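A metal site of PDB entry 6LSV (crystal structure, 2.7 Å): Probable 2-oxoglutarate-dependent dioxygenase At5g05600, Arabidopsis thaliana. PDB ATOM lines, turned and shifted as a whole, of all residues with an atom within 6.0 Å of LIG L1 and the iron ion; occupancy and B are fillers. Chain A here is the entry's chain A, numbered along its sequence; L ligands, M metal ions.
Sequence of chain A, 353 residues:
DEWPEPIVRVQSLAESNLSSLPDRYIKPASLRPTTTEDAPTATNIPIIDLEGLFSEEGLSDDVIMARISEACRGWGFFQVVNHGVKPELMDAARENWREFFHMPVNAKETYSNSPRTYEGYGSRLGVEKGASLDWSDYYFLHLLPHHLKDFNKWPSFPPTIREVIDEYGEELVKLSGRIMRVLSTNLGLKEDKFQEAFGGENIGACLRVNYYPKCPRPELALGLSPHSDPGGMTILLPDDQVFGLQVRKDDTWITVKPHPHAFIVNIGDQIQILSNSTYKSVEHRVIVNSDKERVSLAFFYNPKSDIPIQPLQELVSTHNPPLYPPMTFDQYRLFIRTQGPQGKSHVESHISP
The backbone NH (N) of Arg 294 lies within hydrogen-bond range of the backbone carbonyl oxygen (O) of Tyr 212 (3.0 Å).
The backbone carbonyl oxygen (O) of Ser 296 is in hydrogen-bond range of the backbone NH (N) of Asn 210, at 2.9 Å.
N of Val 286 sits at hydrogen-bond distance from O of Leu 224.
OH of Tyr 212 lies close to ND2 of Asn 210, 3.3 Å away.
The guanidinium group of Arg 208 is in hydrogen-bond range of the side-chain amide oxygen of Asn 210 (2.5 Å).
The side-chain hydroxyl of Ser 296 sits at hydrogen-bond distance from the guanidinium group of Arg 294, at 3.2 Å.
The side-chain carboxylate of Asp 229 sits at hydrogen-bond distance from the side-chain hydroxyl of Thr 234, 2.5 Å away.
The backbone NH (N) of Ala 298 is in hydrogen-bond range of the backbone carbonyl oxygen (O) of Arg 208, at 2.8 Å.
Leu 224 touches LIG L1.
CD1 of Leu 236 touches C4 of LIG L1, at 3.6 Å.
CB of Pro 238 touches O4 of LIG L1 (3.9 Å).
Leu 245 touches LIG L1.
CG2 of Val 286 touches O5 of LIG L1, at 3.4 Å.
CB of Ala 298 touches O1 of LIG L1, at 3.7 Å.
Hydrophobic or aromatic side chains that line LIG L1: Tyr 212, Leu 224, His 227, Leu 236, Pro 238, Leu 245, His 284, Val 286 and Ala 298.
The guanidinium group (NH2) of Arg 294 is in salt-bridge range of an oxygen (O4) of LIG L1.
OH of Tyr 212 lies within hydrogen-bond range of O5 of LIG L1, 2.9 Å away.
The side-chain amide nitrogen (ND2) of Asn 210 is in hydrogen-bond range of an oxygen (O2) of LIG L1.
An oxygen (O5) of LIG L1 is in hydrogen-bond range of the side-chain hydroxyl (OG) of Ser 296 (2.9 Å).
The guanidinium group (NH1) of Arg 208 sits at hydrogen-bond distance from an oxygen (O1) of LG2 L2 (3.0 Å).
The iron ion is bound by O1 of LIG L1 (2.0 Å), NE2 of His 227 (2.4 Å), OD1 of Asp 229 (2.4 Å) and NE2 of His 284 (2.6 Å).
Within 4 Å of the iron ion: His 227, Asp 229 and His 284.
The nearest printed residue that does not touch the iron ion is Leu 224 (4.8 Å).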
ATOM      1  N   ARG A 208      18.077   8.732 -27.286  1.00  0.00           N
ATOM      2  CA  ARG A 208      19.302   8.242 -26.676  1.00  0.00           C
ATOM      3  C   ARG A 208      19.287   6.733 -26.728  1.00  0.00           C
ATOM      4  O   ARG A 208      18.357   6.102 -26.217  1.00  0.00           O
ATOM      5  CB  ARG A 208      19.467   8.724 -25.232  1.00  0.00           C
ATOM      6  CG  ARG A 208      20.396   7.827 -24.426  1.00  0.00           C
ATOM      7  CD  ARG A 208      21.021   8.520 -23.239  1.00  0.00           C
ATOM      8  NE  ARG A 208      21.717   7.558 -22.392  1.00  0.00           N
ATOM      9  CZ  ARG A 208      22.677   7.866 -21.523  1.00  0.00           C
ATOM     10  NH1 ARG A 208      23.064   9.124 -21.392  1.00  0.00           N
ATOM     11  NH2 ARG A 208      23.246   6.924 -20.786  1.00  0.00           N
ATOM     12  N   ASN A 210      21.320   3.252 -25.725  1.00  0.00           N
ATOM     13  CA  ASN A 210      22.223   2.834 -24.661  1.00  0.00           C
ATOM     14  C   ASN A 210      22.824   1.469 -24.990  1.00  0.00           C
ATOM     15  O   ASN A 210      22.099   0.542 -25.368  1.00  0.00           O
ATOM     16  CB  ASN A 210      21.507   2.781 -23.323  1.00  0.00           C
ATOM     17  CG  ASN A 210      20.921   4.118 -22.914  1.00  0.00           C
ATOM     18  OD1 ASN A 210      21.625   5.133 -22.909  1.00  0.00           O
ATOM     19  ND2 ASN A 210      19.643   4.127 -22.570  1.00  0.00           N
ATOM     20  N   TYR A 212      25.101  -1.547 -23.335  1.00  0.00           N
ATOM     21  CA  TYR A 212      25.596  -2.126 -22.082  1.00  0.00           C
ATOM     22  C   TYR A 212      26.436  -3.348 -22.408  1.00  0.00           C
ATOM     23  O   TYR A 212      25.903  -4.469 -22.513  1.00  0.00           O
ATOM     24  CB  TYR A 212      24.428  -2.502 -21.161  1.00  0.00           C
ATOM     25  CG  TYR A 212      23.417  -1.390 -20.984  1.00  0.00           C
ATOM     26  CD1 TYR A 212      23.626  -0.379 -20.061  1.00  0.00           C
ATOM     27  CD2 TYR A 212      22.266  -1.341 -21.761  1.00  0.00           C
ATOM     28  CE1 TYR A 212      22.712   0.650 -19.895  1.00  0.00           C
ATOM     29  CE2 TYR A 212      21.344  -0.316 -21.605  1.00  0.00           C
ATOM     30  CZ  TYR A 212      21.570   0.669 -20.674  1.00  0.00           C
ATOM     31  OH  TYR A 212      20.661   1.687 -20.515  1.00  0.00           O
ATOM     32  N   LEU A 224      23.343   1.769 -15.730  1.00  0.00           N
ATOM     33  CA  LEU A 224      22.863   3.142 -15.618  1.00  0.00           C
ATOM     34  C   LEU A 224      22.323   3.332 -14.203  1.00  0.00           C
ATOM     35  O   LEU A 224      21.436   2.596 -13.766  1.00  0.00           O
ATOM     36  CB  LEU A 224      21.781   3.420 -16.657  1.00  0.00           C
ATOM     37  CG  LEU A 224      21.428   4.875 -16.943  1.00  0.00           C
ATOM     38  CD1 LEU A 224      22.684   5.709 -17.156  1.00  0.00           C
ATOM     39  CD2 LEU A 224      20.507   4.948 -18.155  1.00  0.00           C
ATOM     40  N   HIS A 227      17.642   7.072 -11.682  1.00  0.00           N
ATOM     41  CA  HIS A 227      17.204   8.380 -12.149  1.00  0.00           C
ATOM     42  C   HIS A 227      15.764   8.275 -12.632  1.00  0.00           C
ATOM     43  O   HIS A 227      15.283   7.187 -12.988  1.00  0.00           O
ATOM     44  CB  HIS A 227      18.074   8.915 -13.284  1.00  0.00           C
ATOM     45  CG  HIS A 227      17.851   8.217 -14.591  1.00  0.00           C
ATOM     46  ND1 HIS A 227      18.166   6.884 -14.782  1.00  0.00           N
ATOM     47  CD2 HIS A 227      17.332   8.654 -15.751  1.00  0.00           C
ATOM     48  CE1 HIS A 227      17.850   6.533 -16.015  1.00  0.00           C
ATOM     49  NE2 HIS A 227      17.346   7.590 -16.627  1.00  0.00           N
ATOM     50  N   SER A 228      15.086   9.416 -12.663  1.00  0.00           N
ATOM     51  CA  SER A 228      13.888   9.594 -13.465  1.00  0.00           C
ATOM     52  C   SER A 228      14.245  10.462 -14.661  1.00  0.00           C
ATOM     53  O   SER A 228      15.169  11.286 -14.598  1.00  0.00           O
ATOM     54  CB  SER A 228      12.752  10.228 -12.652  1.00  0.00           C
ATOM     55  OG  SER A 228      13.138  11.463 -12.083  1.00  0.00           O
ATOM     56  N   ASP A 229      13.522  10.268 -15.758  1.00  0.00           N
ATOM     57  CA  ASP A 229      13.808  11.026 -16.968  1.00  0.00           C
ATOM     58  C   ASP A 229      13.386  12.478 -16.785  1.00  0.00           C
ATOM     59  O   ASP A 229      12.269  12.736 -16.316  1.00  0.00           O
ATOM     60  CB  ASP A 229      13.090  10.401 -18.160  1.00  0.00           C
ATOM     61  CG  ASP A 229      13.631   9.029 -18.493  1.00  0.00           C
ATOM     62  OD1 ASP A 229      14.844   8.816 -18.322  1.00  0.00           O
ATOM     63  OD2 ASP A 229      12.838   8.165 -18.925  1.00  0.00           O
ATOM     64  N   THR A 234       8.963   9.217 -21.761  1.00  0.00           N
ATOM     65  CA  THR A 234       9.920   8.397 -22.477  1.00  0.00           C
ATOM     66  C   THR A 234       9.215   7.184 -23.066  1.00  0.00           C
ATOM     67  O   THR A 234       8.443   6.519 -22.365  1.00  0.00           O
ATOM     68  CB  THR A 234      11.059   7.943 -21.555  1.00  0.00           C
ATOM     69  OG1 THR A 234      11.638   9.081 -20.911  1.00  0.00           O
ATOM     70  CG2 THR A 234      12.138   7.220 -22.364  1.00  0.00           C
ATOM     71  N   LEU A 236      10.327   3.739 -24.309  1.00  0.00           N
ATOM     72  CA  LEU A 236      11.521   2.917 -24.152  1.00  0.00           C
ATOM     73  C   LEU A 236      11.342   1.600 -24.886  1.00  0.00           C
ATOM     74  O   LEU A 236      10.340   0.898 -24.686  1.00  0.00           O
ATOM     75  CB  LEU A 236      11.787   2.657 -22.658  1.00  0.00           C
ATOM     76  CG  LEU A 236      12.948   1.764 -22.209  1.00  0.00           C
ATOM     77  CD1 LEU A 236      14.278   2.280 -22.732  1.00  0.00           C
ATOM     78  CD2 LEU A 236      12.970   1.691 -20.682  1.00  0.00           C
ATOM     79  N   LEU A 237      12.296   1.274 -25.759  1.00  0.00           N
ATOM     80  CA  LEU A 237      12.350  -0.030 -26.409  1.00  0.00           C
ATOM     81  C   LEU A 237      13.482  -0.815 -25.762  1.00  0.00           C
ATOM     82  O   LEU A 237      14.646  -0.706 -26.187  1.00  0.00           O
ATOM     83  CB  LEU A 237      12.562   0.094 -27.912  1.00  0.00           C
ATOM     84  CG  LEU A 237      12.587  -1.237 -28.673  1.00  0.00           C
ATOM     85  CD1 LEU A 237      11.408  -2.113 -28.256  1.00  0.00           C
ATOM     86  CD2 LEU A 237      12.595  -1.022 -30.178  1.00  0.00           C
ATOM     87  N   PRO A 238      13.209  -1.593 -24.722  1.00  0.00           N
ATOM     88  CA  PRO A 238      14.286  -2.334 -24.049  1.00  0.00           C
ATOM     89  C   PRO A 238      14.739  -3.519 -24.880  1.00  0.00           C
ATOM     90  O   PRO A 238      14.045  -3.976 -25.788  1.00  0.00           O
ATOM     91  CB  PRO A 238      13.643  -2.779 -22.735  1.00  0.00           C
ATOM     92  CG  PRO A 238      12.186  -2.853 -23.041  1.00  0.00           C
ATOM     93  CD  PRO A 238      11.889  -1.835 -24.107  1.00  0.00           C
ATOM     94  N   ASP A 239      15.930  -3.997 -24.556  1.00  0.00           N
ATOM     95  CA  ASP A 239      16.535  -5.105 -25.295  1.00  0.00           C
ATOM     96  C   ASP A 239      15.604  -6.308 -25.280  1.00  0.00           C
ATOM     97  O   ASP A 239      15.203  -6.794 -24.219  1.00  0.00           O
ATOM     98  CB  ASP A 239      17.888  -5.464 -24.692  1.00  0.00           C
ATOM     99  CG  ASP A 239      18.704  -6.382 -25.587  1.00  0.00           C
ATOM    100  OD1 ASP A 239      18.391  -7.586 -25.629  1.00  0.00           O
ATOM    101  OD2 ASP A 239      19.639  -5.886 -26.251  1.00  0.00           O
ATOM    102  N   GLY A 244      17.594  -6.406 -17.802  1.00  0.00           N
ATOM    103  CA  GLY A 244      18.511  -5.455 -17.212  1.00  0.00           C
ATOM    104  C   GLY A 244      17.823  -4.211 -16.679  1.00  0.00           C
ATOM    105  O   GLY A 244      18.301  -3.589 -15.729  1.00  0.00           O
ATOM    106  N   LEU A 245      16.696  -3.841 -17.280  1.00  0.00           N
ATOM    107  CA  LEU A 245      15.961  -2.675 -16.827  1.00  0.00           C
ATOM    108  C   LEU A 245      15.264  -2.972 -15.502  1.00  0.00           C
ATOM    109  O   LEU A 245      14.601  -4.002 -15.364  1.00  0.00           O
ATOM    110  CB  LEU A 245      14.949  -2.243 -17.885  1.00  0.00           C
ATOM    111  CG  LEU A 245      13.935  -1.196 -17.424  1.00  0.00           C
ATOM    112  CD1 LEU A 245      14.584   0.170 -17.332  1.00  0.00           C
ATOM    113  CD2 LEU A 245      12.758  -1.178 -18.372  1.00  0.00           C
ATOM    114  N   ASN A 266       7.279   5.726 -20.065  1.00  0.00           N
ATOM    115  CA  ASN A 266       7.737   6.265 -18.799  1.00  0.00           C
ATOM    116  C   ASN A 266       7.193   7.671 -18.618  1.00  0.00           C
ATOM    117  O   ASN A 266       7.354   8.523 -19.502  1.00  0.00           O
ATOM    118  CB  ASN A 266       9.269   6.292 -18.711  1.00  0.00           C
ATOM    119  CG  ASN A 266       9.868   4.927 -18.471  1.00  0.00           C
ATOM    120  OD1 ASN A 266       9.170   3.984 -18.089  1.00  0.00           O
ATOM    121  ND2 ASN A 266      11.172   4.813 -18.674  1.00  0.00           N
ATOM    122  N   HIS A 284      14.221   4.487 -12.535  1.00  0.00           N
ATOM    123  CA  HIS A 284      14.733   3.242 -13.087  1.00  0.00           C
ATOM    124  C   HIS A 284      16.253   3.250 -13.099  1.00  0.00           C
ATOM    125  O   HIS A 284      16.905   4.276 -12.916  1.00  0.00           O
ATOM    126  CB  HIS A 284      14.185   2.992 -14.503  1.00  0.00           C
ATOM    127  CG  HIS A 284      14.078   4.221 -15.338  1.00  0.00           C
ATOM    128  ND1 HIS A 284      13.070   5.147 -15.179  1.00  0.00           N
ATOM    129  CD2 HIS A 284      14.840   4.679 -16.364  1.00  0.00           C
ATOM    130  CE1 HIS A 284      13.225   6.128 -16.052  1.00  0.00           C
ATOM    131  NE2 HIS A 284      14.292   5.861 -16.783  1.00  0.00           N
ATOM    132  N   ARG A 285      16.801   2.052 -13.307  1.00  0.00           N
ATOM    133  CA  ARG A 285      18.237   1.823 -13.396  1.00  0.00           C
ATOM    134  C   ARG A 285      18.430   0.572 -14.240  1.00  0.00           C
ATOM    135  O   ARG A 285      17.513  -0.223 -14.443  1.00  0.00           O
ATOM    136  CB  ARG A 285      18.867   1.657 -12.019  1.00  0.00           C
ATOM    137  CG  ARG A 285      18.588   0.313 -11.374  1.00  0.00           C
ATOM    138  CD  ARG A 285      19.242   0.171 -10.010  1.00  0.00           C
ATOM    139  NE  ARG A 285      19.133  -1.198  -9.516  1.00  0.00           N
ATOM    140  CZ  ARG A 285      19.523  -1.593  -8.307  1.00  0.00           C
ATOM    141  NH1 ARG A 285      20.051  -0.737  -7.458  1.00  0.00           N
ATOM    142  NH2 ARG A 285      19.382  -2.869  -7.952  1.00  0.00           N
ATOM    143  N   VAL A 286      19.649   0.396 -14.747  1.00  0.00           N
ATOM    144  CA  VAL A 286      19.989  -0.757 -15.577  1.00  0.00           C
ATOM    145  C   VAL A 286      21.088  -1.546 -14.870  1.00  0.00           C
ATOM    146  O   VAL A 286      22.078  -0.964 -14.413  1.00  0.00           O
ATOM    147  CB  VAL A 286      20.425  -0.342 -16.990  1.00  0.00           C
ATOM    148  CG1 VAL A 286      20.529  -1.570 -17.889  1.00  0.00           C
ATOM    149  CG2 VAL A 286      19.445   0.662 -17.579  1.00  0.00           C
ATOM    150  N   ARG A 294      23.482  -5.617 -23.944  1.00  0.00           N
ATOM    151  CA  ARG A 294      22.122  -5.119 -24.095  1.00  0.00           C
ATOM    152  C   ARG A 294      22.156  -3.900 -24.996  1.00  0.00           C
ATOM    153  O   ARG A 294      23.158  -3.185 -25.064  1.00  0.00           O
ATOM    154  CB  ARG A 294      21.472  -4.762 -22.741  1.00  0.00           C
ATOM    155  CG  ARG A 294      20.954  -5.951 -21.942  1.00  0.00           C
ATOM    156  CD  ARG A 294      20.164  -5.525 -20.702  1.00  0.00           C
ATOM    157  NE  ARG A 294      18.786  -5.157 -21.000  1.00  0.00           N
ATOM    158  CZ  ARG A 294      18.326  -3.907 -21.012  1.00  0.00           C
ATOM    159  NH1 ARG A 294      19.133  -2.891 -20.748  1.00  0.00           N
ATOM    160  NH2 ARG A 294      17.049  -3.670 -21.309  1.00  0.00           N
ATOM    161  N   VAL A 295      21.051  -3.666 -25.687  1.00  0.00           N
ATOM    162  CA  VAL A 295      20.852  -2.451 -26.478  1.00  0.00           C
ATOM    163  C   VAL A 295      19.423  -1.981 -26.258  1.00  0.00           C
ATOM    164  O   VAL A 295      18.476  -2.735 -26.515  1.00  0.00           O
ATOM    165  CB  VAL A 295      21.105  -2.679 -27.977  1.00  0.00           C
ATOM    166  CG1 VAL A 295      20.444  -1.593 -28.798  1.00  0.00           C
ATOM    167  CG2 VAL A 295      22.604  -2.740 -28.264  1.00  0.00           C
ATOM    168  N   SER A 296      19.264  -0.760 -25.765  1.00  0.00           N
ATOM    169  CA  SER A 296      17.952  -0.195 -25.513  1.00  0.00           C
ATOM    170  C   SER A 296      17.852   1.191 -26.127  1.00  0.00           C
ATOM    171  O   SER A 296      18.838   1.931 -26.203  1.00  0.00           O
ATOM    172  CB  SER A 296      17.643  -0.132 -24.012  1.00  0.00           C
ATOM    173  OG  SER A 296      18.007  -1.352 -23.378  1.00  0.00           O
ATOM    174  N   ALA A 298      15.855   4.829 -26.048  1.00  0.00           N
ATOM    175  CA  ALA A 298      15.075   5.739 -25.220  1.00  0.00           C
ATOM    176  C   ALA A 298      14.674   6.937 -26.059  1.00  0.00           C
ATOM    177  O   ALA A 298      15.515   7.781 -26.402  1.00  0.00           O
ATOM    178  CB  ALA A 298      15.868   6.172 -23.985  1.00  0.00           C
ATOM    179  N   PHE A 300      12.626  10.381 -26.137  1.00  0.00           N
ATOM    180  CA  PHE A 300      12.176  11.393 -25.193  1.00  0.00           C
ATOM    181  C   PHE A 300      11.215  12.352 -25.894  1.00  0.00           C
ATOM    182  O   PHE A 300      11.568  12.956 -26.905  1.00  0.00           O
ATOM    183  CB  PHE A 300      13.356  12.161 -24.604  1.00  0.00           C
ATOM    184  CG  PHE A 300      14.397  11.296 -23.958  1.00  0.00           C
ATOM    185  CD1 PHE A 300      14.081  10.513 -22.849  1.00  0.00           C
ATOM    186  CD2 PHE A 300      15.689  11.262 -24.450  1.00  0.00           C
ATOM    187  CE1 PHE A 300      15.052   9.714 -22.247  1.00  0.00           C
ATOM    188  CE2 PHE A 300      16.648  10.469 -23.851  1.00  0.00           C
ATOM    189  CZ  PHE A 300      16.330   9.694 -22.754  1.00  0.00           C
HETATM  190  C1  LIG L   1      17.135   5.189 -20.333  1.00  0.00           C
HETATM  191  O1  LIG L   1      16.074   5.852 -20.304  1.00  0.00           O
HETATM  192  O2  LIG L   1      18.174   5.701 -20.846  1.00  0.00           O
HETATM  193  C2  LIG L   1      17.169   3.782 -19.732  1.00  0.00           C
HETATM  194  O3  LIG L   1      16.951   3.652 -18.569  1.00  0.00           O
HETATM  195  C3  LIG L   1      17.475   2.531 -20.574  1.00  0.00           C
HETATM  196  C4  LIG L   1      16.607   1.366 -20.076  1.00  0.00           C
HETATM  197  C5  LIG L   1      17.166   0.024 -20.559  1.00  0.00           C
HETATM  198  O4  LIG L   1      16.409  -0.959 -20.752  1.00  0.00           O
HETATM  199  O5  LIG L   1      18.397  -0.091 -20.770  1.00  0.00           O
HETATM  200  O1  LG2 L   2      21.833  11.646 -22.384  1.00  0.00           O
HETATM  201  O2  LG2 L   2      17.353  16.150 -22.623  1.00  0.00           O
HETATM  202  O3  LG2 L   2      18.896  17.334 -21.657  1.00  0.00           O
HETATM  203  C1  LG2 L   2      19.624  14.190 -22.041  1.00  0.00           C
HETATM  204  C2  LG2 L   2      20.326  12.905 -21.324  1.00  0.00           C
HETATM  205  C3  LG2 L   2      20.833  15.014 -22.567  1.00  0.00           C
HETATM  206  C4  LG2 L   2      21.924  14.169 -22.550  1.00  0.00           C
HETATM  207  C5  LG2 L   2      21.367  12.698 -22.081  1.00  0.00           C
HETATM  208  C6  LG2 L   2      19.363  11.637 -21.318  1.00  0.00           C
HETATM  209  C7  LG2 L   2      18.850  14.963 -21.129  1.00  0.00           C
HETATM  210  C8  LG2 L   2      18.472  11.660 -20.078  1.00  0.00           C
HETATM  211  C9  LG2 L   2      18.334  16.216 -21.839  1.00  0.00           C
HETATM  212  C10 LG2 L   2      18.333  10.604 -19.299  1.00  0.00           C
HETATM  213  C11 LG2 L   2      19.053   9.290 -19.606  1.00  0.00           C
HETATM  214  C12 LG2 L   2      19.818   8.824 -18.371  1.00  0.00           C
HETATM  215 FE    FE M   1      16.092   6.714 -18.480  1.00  0.00          FE
